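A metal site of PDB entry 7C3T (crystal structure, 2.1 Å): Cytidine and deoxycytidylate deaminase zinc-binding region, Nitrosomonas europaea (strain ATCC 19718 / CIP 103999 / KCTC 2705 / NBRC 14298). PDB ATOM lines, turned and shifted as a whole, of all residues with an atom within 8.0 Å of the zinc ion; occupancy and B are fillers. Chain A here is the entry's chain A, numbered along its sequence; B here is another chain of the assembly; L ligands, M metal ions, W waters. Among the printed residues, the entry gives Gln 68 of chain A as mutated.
A nitrogen (N6) of the ligand is in hydrogen-bond range of the side-chain carboxylate (OE1) of Glu 81 (2.7 Å). The side-chain carboxylate (OE1) of Glu 145 lies within hydrogen-bond range of a nitrogen (N2) of the ligand, at 3.2 Å. The backbone NH (N) of Ala 80 lies within hydrogen-bond range of a nitrogen (N5) of the ligand. A nitrogen (N2) of the ligand lies within hydrogen-bond range of the backbone carbonyl oxygen (O) of Asp 144 (3.1 Å). An oxygen (O1) of the ligand is in hydrogen-bond range of the side-chain amide oxygen (OE1) of Gln 68, 2.7 Å away.
The side-chain sulfur (SG) of Cys 117 sits close to the side-chain carboxylate (OE2) of Glu 81 (3.7 Å). The side-chain sulfur (SG) of Cys 114 lies close to the backbone NH (N) of Met 116 (3.5 Å). The side-chain sulfur (SG) of Cys 114 lies close to the indole nitrogen (NE1) of Trp 123 of chain B (3.4 Å). N of Cys 114 sits at hydrogen-bond distance from OE1 of Glu 145, at 3.2 Å.
Residues that only touch the zinc ion: Glu 81 (3.8 Å) and Met 116 (3.8 Å).
Water W1 is bound to the zinc ion (2.0 Å). A ring nitrogen (ND1) of His 79 binds the zinc ion (2.1 Å). SG of Cys 117 is bound to the zinc ion, at 2.3 Å. The side-chain sulfur (SG) of Cys 114 binds the zinc ion (2.3 Å). The zinc ion has four donor atoms within binding distance.
Water W1 lies within hydrogen-bond range of the side-chain carboxylate of Glu 81 (2.5 Å), the backbone NH of Cys 114 (2.8 Å) and a nitrogen (N1) of the ligand (2.9 Å).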
ATOM      1  N   PHE A  50      -0.536  19.477  11.014  1.00  0.00           N
ATOM      2  CA  PHE A  50      -1.330  18.986   9.900  1.00  0.00           C
ATOM      3  C   PHE A  50      -1.147  17.520   9.763  1.00  0.00           C
ATOM      4  O   PHE A  50       0.002  16.979   9.855  1.00  0.00           O
ATOM      5  CB  PHE A  50      -0.895  19.637   8.600  1.00  0.00           C
ATOM      6  CG  PHE A  50      -0.989  21.117   8.637  1.00  0.00           C
ATOM      7  CD1 PHE A  50      -2.213  21.727   8.439  1.00  0.00           C
ATOM      8  CD2 PHE A  50       0.123  21.901   8.879  1.00  0.00           C
ATOM      9  CE1 PHE A  50      -2.332  23.130   8.493  1.00  0.00           C
ATOM     10  CE2 PHE A  50       0.016  23.295   8.916  1.00  0.00           C
ATOM     11  CZ  PHE A  50      -1.196  23.909   8.737  1.00  0.00           C
ATOM     12  N   GLN A  68       2.540  16.514   8.042  1.00  0.00           N
ATOM     13  CA  GLN A  68       3.495  17.451   7.519  1.00  0.00           C
ATOM     14  C   GLN A  68       4.918  17.203   8.032  1.00  0.00           C
ATOM     15  O   GLN A  68       5.198  17.289   9.236  1.00  0.00           O
ATOM     16  CB  GLN A  68       3.093  18.844   7.906  1.00  0.00           C
ATOM     17  CG  GLN A  68       3.891  19.863   7.106  1.00  0.00           C
ATOM     18  CD  GLN A  68       4.528  20.944   7.881  1.00  0.00           C
ATOM     19  OE1 GLN A  68       4.076  22.080   7.790  1.00  0.00           O
ATOM     20  NE2 GLN A  68       5.665  20.616   8.620  1.00  0.00           N
ATOM     21  N   VAL A  70       7.681  18.868   6.519  1.00  0.00           N
ATOM     22  CA  VAL A  70       8.427  19.835   5.732  1.00  0.00           C
ATOM     23  C   VAL A  70       9.842  20.101   6.295  1.00  0.00           C
ATOM     24  O   VAL A  70      10.842  19.958   5.560  1.00  0.00           O
ATOM     25  CB  VAL A  70       7.575  21.113   5.553  1.00  0.00           C
ATOM     26  CG1 VAL A  70       8.419  22.342   5.157  1.00  0.00           C
ATOM     27  CG2 VAL A  70       6.464  20.846   4.541  1.00  0.00           C
ATOM     28  N   SER A  76       9.660  21.036   1.036  1.00  0.00           N
ATOM     29  CA  SER A  76       8.515  21.916   1.117  1.00  0.00           C
ATOM     30  C   SER A  76       7.280  21.258   0.538  1.00  0.00           C
ATOM     31  O   SER A  76       6.161  21.728   0.838  1.00  0.00           O
ATOM     32  CB  SER A  76       8.789  23.235   0.398  1.00  0.00           C
ATOM     33  OG  SER A  76       9.143  22.963  -0.946  1.00  0.00           O
ATOM     34  N   ALA A  77       7.462  20.220  -0.306  1.00  0.00           N
ATOM     35  CA  ALA A  77       6.317  19.474  -0.816  1.00  0.00           C
ATOM     36  C   ALA A  77       5.698  18.496   0.189  1.00  0.00           C
ATOM     37  O   ALA A  77       4.682  17.934  -0.135  1.00  0.00           O
ATOM     38  CB  ALA A  77       6.692  18.728  -2.086  1.00  0.00           C
ATOM     39  N   ALA A  78       6.322  18.244   1.335  1.00  0.00           N
ATOM     40  CA  ALA A  78       5.862  17.197   2.300  1.00  0.00           C
ATOM     41  C   ALA A  78       4.751  17.648   3.256  1.00  0.00           C
ATOM     42  O   ALA A  78       4.859  17.554   4.491  1.00  0.00           O
ATOM     43  CB  ALA A  78       7.047  16.699   3.113  1.00  0.00           C
ATOM     44  N   HIS A  79       3.697  18.169   2.677  1.00  0.00           N
ATOM     45  CA  HIS A  79       2.459  18.440   3.357  1.00  0.00           C
ATOM     46  C   HIS A  79       1.748  17.111   3.649  1.00  0.00           C
ATOM     47  O   HIS A  79       1.982  16.075   2.983  1.00  0.00           O
ATOM     48  CB  HIS A  79       1.581  19.320   2.475  1.00  0.00           C
ATOM     49  CG  HIS A  79       2.048  20.720   2.372  1.00  0.00           C
ATOM     50  ND1 HIS A  79       1.241  21.733   1.905  1.00  0.00           N
ATOM     51  CD2 HIS A  79       3.227  21.296   2.674  1.00  0.00           C
ATOM     52  CE1 HIS A  79       1.887  22.874   1.955  1.00  0.00           C
ATOM     53  NE2 HIS A  79       3.087  22.646   2.437  1.00  0.00           N
ATOM     54  N   ALA A  80       0.859  17.160   4.624  1.00  0.00           N
ATOM     55  CA  ALA A  80       0.157  15.978   5.101  1.00  0.00           C
ATOM     56  C   ALA A  80      -0.585  15.198   3.942  1.00  0.00           C
ATOM     57  O   ALA A  80      -0.450  13.980   3.840  1.00  0.00           O
ATOM     58  CB  ALA A  80      -0.806  16.377   6.194  1.00  0.00           C
ATOM     59  N   GLU A  81      -1.232  15.953   3.043  1.00  0.00           N
ATOM     60  CA  GLU A  81      -2.030  15.473   1.951  1.00  0.00           C
ATOM     61  C   GLU A  81      -1.185  14.733   0.909  1.00  0.00           C
ATOM     62  O   GLU A  81      -1.540  13.633   0.496  1.00  0.00           O
ATOM     63  CB  GLU A  81      -2.846  16.626   1.291  1.00  0.00           C
ATOM     64  CG  GLU A  81      -3.744  17.420   2.238  1.00  0.00           C
ATOM     65  CD  GLU A  81      -3.075  18.674   2.858  1.00  0.00           C
ATOM     66  OE1 GLU A  81      -2.005  18.565   3.573  1.00  0.00           O
ATOM     67  OE2 GLU A  81      -3.620  19.789   2.588  1.00  0.00           O
ATOM     68  N   ILE A  82      -0.040  15.323   0.562  1.00  0.00           N
ATOM     69  CA  ILE A  82       0.922  14.689  -0.339  1.00  0.00           C
ATOM     70  C   ILE A  82       1.415  13.384   0.189  1.00  0.00           C
ATOM     71  O   ILE A  82       1.466  12.392  -0.611  1.00  0.00           O
ATOM     72  CB  ILE A  82       2.175  15.571  -0.677  1.00  0.00           C
ATOM     73  CG1 ILE A  82       1.747  16.919  -1.234  1.00  0.00           C
ATOM     74  CG2 ILE A  82       3.126  14.879  -1.656  1.00  0.00           C
ATOM     75  CD1 ILE A  82       0.746  16.876  -2.333  1.00  0.00           C
ATOM     76  N   ALA A 111      -7.050  20.116   7.816  1.00  0.00           N
ATOM     77  CA  ALA A 111      -7.327  21.472   7.342  1.00  0.00           C
ATOM     78  C   ALA A 111      -7.574  21.498   5.843  1.00  0.00           C
ATOM     79  O   ALA A 111      -7.098  20.624   5.115  1.00  0.00           O
ATOM     80  CB  ALA A 111      -6.144  22.370   7.677  1.00  0.00           C
ATOM     81  N   GLU A 112      -8.281  22.535   5.397  1.00  0.00           N
ATOM     82  CA  GLU A 112      -8.511  22.714   3.985  1.00  0.00           C
ATOM     83  C   GLU A 112      -7.190  22.764   3.222  1.00  0.00           C
ATOM     84  O   GLU A 112      -6.166  23.269   3.743  1.00  0.00           O
ATOM     85  CB  GLU A 112      -9.339  23.963   3.737  1.00  0.00           C
ATOM     86  CG  GLU A 112     -10.789  23.719   4.153  1.00  0.00           C
ATOM     87  CD  GLU A 112     -11.650  24.948   4.035  1.00  0.00           C
ATOM     88  OE1 GLU A 112     -11.103  26.007   3.613  1.00  0.00           O
ATOM     89  OE2 GLU A 112     -12.857  24.829   4.422  1.00  0.00           O
ATOM     90  N   PRO A 113      -7.170  22.199   1.996  1.00  0.00           N
ATOM     91  CA  PRO A 113      -5.884  22.041   1.326  1.00  0.00           C
ATOM     92  C   PRO A 113      -5.290  23.349   0.774  1.00  0.00           C
ATOM     93  O   PRO A 113      -6.019  24.216   0.317  1.00  0.00           O
ATOM     94  CB  PRO A 113      -6.213  21.047   0.201  1.00  0.00           C
ATOM     95  CG  PRO A 113      -7.647  21.327  -0.099  1.00  0.00           C
ATOM     96  CD  PRO A 113      -8.231  21.509   1.272  1.00  0.00           C
ATOM     97  N   CYS A 114      -3.966  23.477   0.774  1.00  0.00           N
ATOM     98  CA  CYS A 114      -3.346  24.618   0.087  1.00  0.00           C
ATOM     99  C   CYS A 114      -3.437  24.381  -1.422  1.00  0.00           C
ATOM    100  O   CYS A 114      -3.920  23.311  -1.893  1.00  0.00           O
ATOM    101  CB  CYS A 114      -1.892  24.801   0.496  1.00  0.00           C
ATOM    102  SG  CYS A 114      -0.787  23.554  -0.215  1.00  0.00           S
ATOM    103  N   VAL A 115      -2.998  25.363  -2.195  1.00  0.00           N
ATOM    104  CA  VAL A 115      -3.127  25.285  -3.647  1.00  0.00           C
ATOM    105  C   VAL A 115      -2.341  24.058  -4.224  1.00  0.00           C
ATOM    106  O   VAL A 115      -2.808  23.395  -5.131  1.00  0.00           O
ATOM    107  CB  VAL A 115      -2.794  26.639  -4.342  1.00  0.00           C
ATOM    108  CG1 VAL A 115      -1.356  27.053  -4.112  1.00  0.00           C
ATOM    109  CG2 VAL A 115      -3.083  26.564  -5.826  1.00  0.00           C
ATOM    110  N   MET A 116      -1.171  23.737  -3.649  1.00  0.00           N
ATOM    111  CA  MET A 116      -0.416  22.575  -4.056  1.00  0.00           C
ATOM    112  C   MET A 116      -1.260  21.291  -3.881  1.00  0.00           C
ATOM    113  O   MET A 116      -1.478  20.506  -4.841  1.00  0.00           O
ATOM    114  CB  MET A 116       0.827  22.450  -3.222  1.00  0.00           C
ATOM    115  CG  MET A 116       1.723  21.332  -3.605  1.00  0.00           C
ATOM    116  SD  MET A 116       3.246  21.204  -2.662  1.00  0.00           S
ATOM    117  CE  MET A 116       2.531  21.024  -1.042  1.00  0.00           C
ATOM    118  N   CYS A 117      -1.744  21.118  -2.648  1.00  0.00           N
ATOM    119  CA  CYS A 117      -2.464  19.915  -2.274  1.00  0.00           C
ATOM    120  C   CYS A 117      -3.795  19.813  -2.975  1.00  0.00           C
ATOM    121  O   CYS A 117      -4.215  18.724  -3.321  1.00  0.00           O
ATOM    122  CB  CYS A 117      -2.603  19.845  -0.762  1.00  0.00           C
ATOM    123  SG  CYS A 117      -0.990  19.656   0.032  1.00  0.00           S
ATOM    124  N   PHE A 118      -4.459  20.936  -3.185  1.00  0.00           N
ATOM    125  CA  PHE A 118      -5.633  21.023  -4.040  1.00  0.00           C
ATOM    126  C   PHE A 118      -5.436  20.306  -5.383  1.00  0.00           C
ATOM    127  O   PHE A 118      -6.180  19.380  -5.750  1.00  0.00           O
ATOM    128  CB  PHE A 118      -5.942  22.494  -4.202  1.00  0.00           C
ATOM    129  CG  PHE A 118      -6.943  22.812  -5.256  1.00  0.00           C
ATOM    130  CD1 PHE A 118      -8.290  22.579  -5.046  1.00  0.00           C
ATOM    131  CD2 PHE A 118      -6.563  23.398  -6.430  1.00  0.00           C
ATOM    132  CE1 PHE A 118      -9.226  22.930  -5.981  1.00  0.00           C
ATOM    133  CE2 PHE A 118      -7.500  23.716  -7.391  1.00  0.00           C
ATOM    134  CZ  PHE A 118      -8.841  23.495  -7.154  1.00  0.00           C
ATOM    135  N   ALA A 120      -3.005  18.225  -6.058  1.00  0.00           N
ATOM    136  CA  ALA A 120      -2.670  16.818  -5.785  1.00  0.00           C
ATOM    137  C   ALA A 120      -3.924  15.960  -5.561  1.00  0.00           C
ATOM    138  O   ALA A 120      -4.028  14.791  -6.010  1.00  0.00           O
ATOM    139  CB  ALA A 120      -1.731  16.723  -4.558  1.00  0.00           C
ATOM    140  N   ASP A 144       0.124  29.819   5.222  1.00  0.00           N
ATOM    141  CA  ASP A 144      -0.453  30.385   3.996  1.00  0.00           C
ATOM    142  C   ASP A 144      -1.093  29.261   3.205  1.00  0.00           C
ATOM    143  O   ASP A 144      -0.498  28.225   3.083  1.00  0.00           O
ATOM    144  CB  ASP A 144       0.731  30.988   3.224  1.00  0.00           C
ATOM    145  CG  ASP A 144       0.350  31.845   2.021  1.00  0.00           C
ATOM    146  OD1 ASP A 144      -0.805  32.161   1.649  1.00  0.00           O
ATOM    147  OD2 ASP A 144       1.335  32.232   1.447  1.00  0.00           O
ATOM    148  N   GLU A 145      -2.301  29.454   2.693  1.00  0.00           N
ATOM    149  CA  GLU A 145      -2.935  28.489   1.800  1.00  0.00           C
ATOM    150  C   GLU A 145      -2.582  28.742   0.327  1.00  0.00           C
ATOM    151  O   GLU A 145      -2.781  27.854  -0.537  1.00  0.00           O
ATOM    152  CB  GLU A 145      -4.458  28.480   1.949  1.00  0.00           C
ATOM    153  CG  GLU A 145      -4.948  27.996   3.331  1.00  0.00           C
ATOM    154  CD  GLU A 145      -4.992  26.478   3.490  1.00  0.00           C
ATOM    155  OE1 GLU A 145      -4.047  25.746   3.055  1.00  0.00           O
ATOM    156  OE2 GLU A 145      -5.984  25.978   4.088  1.00  0.00           O
ATOM    157  N   GLY B 119       1.674  25.584  -6.974  1.00  0.00           N
ATOM    158  CA  GLY B 119       1.771  25.574  -5.510  1.00  0.00           C
ATOM    159  C   GLY B 119       3.168  25.155  -4.999  1.00  0.00           C
ATOM    160  O   GLY B 119       3.788  25.854  -4.210  1.00  0.00           O
ATOM    161  N   TRP B 123       5.960  27.463  -2.559  1.00  0.00           N
ATOM    162  CA  TRP B 123       6.484  27.055  -1.250  1.00  0.00           C
ATOM    163  C   TRP B 123       7.950  26.721  -1.268  1.00  0.00           C
ATOM    164  O   TRP B 123       8.530  26.627  -0.240  1.00  0.00           O
ATOM    165  CB  TRP B 123       5.750  25.799  -0.703  1.00  0.00           C
ATOM    166  CG  TRP B 123       4.248  25.909  -0.684  1.00  0.00           C
ATOM    167  CD1 TRP B 123       3.367  24.913  -1.029  1.00  0.00           C
ATOM    168  CD2 TRP B 123       3.470  27.033  -0.304  1.00  0.00           C
ATOM    169  NE1 TRP B 123       2.056  25.371  -0.883  1.00  0.00           N
ATOM    170  CE2 TRP B 123       2.105  26.662  -0.433  1.00  0.00           C
ATOM    171  CE3 TRP B 123       3.786  28.321   0.133  1.00  0.00           C
ATOM    172  CZ2 TRP B 123       1.048  27.562  -0.188  1.00  0.00           C
ATOM    173  CZ3 TRP B 123       2.752  29.197   0.413  1.00  0.00           C
ATOM    174  CH2 TRP B 123       1.389  28.804   0.249  1.00  0.00           C
HETATM  175  C1  LIG L   1      -0.678  21.923   5.008  1.00  0.00           C
HETATM  176  N1  LIG L   1      -1.319  23.115   4.666  1.00  0.00           N
HETATM  177  C2  LIG L   1      -0.652  24.316   4.778  1.00  0.00           C
HETATM  178  N2  LIG L   1      -1.232  25.491   4.458  1.00  0.00           N
HETATM  179  N3  LIG L   1       0.623  24.410   5.230  1.00  0.00           N
HETATM  180  C3  LIG L   1       1.308  23.302   5.601  1.00  0.00           C
HETATM  181  O1  LIG L   1       2.500  23.453   6.091  1.00  0.00           O
HETATM  182  C4  LIG L   1       0.712  21.944   5.519  1.00  0.00           C
HETATM  183  N4  LIG L   1       1.064  20.664   5.787  1.00  0.00           N
HETATM  184  N5  LIG L   1       0.062  19.789   5.497  1.00  0.00           N
HETATM  185  N6  LIG L   1      -1.089  20.602   5.020  1.00  0.00           N
HETATM  186 ZN    ZN M   1      -0.639  21.634   1.047  1.00  0.00          ZN
HETATM  187  O   HOH W   1      -2.232  21.817   2.223  1.00  0.00           O
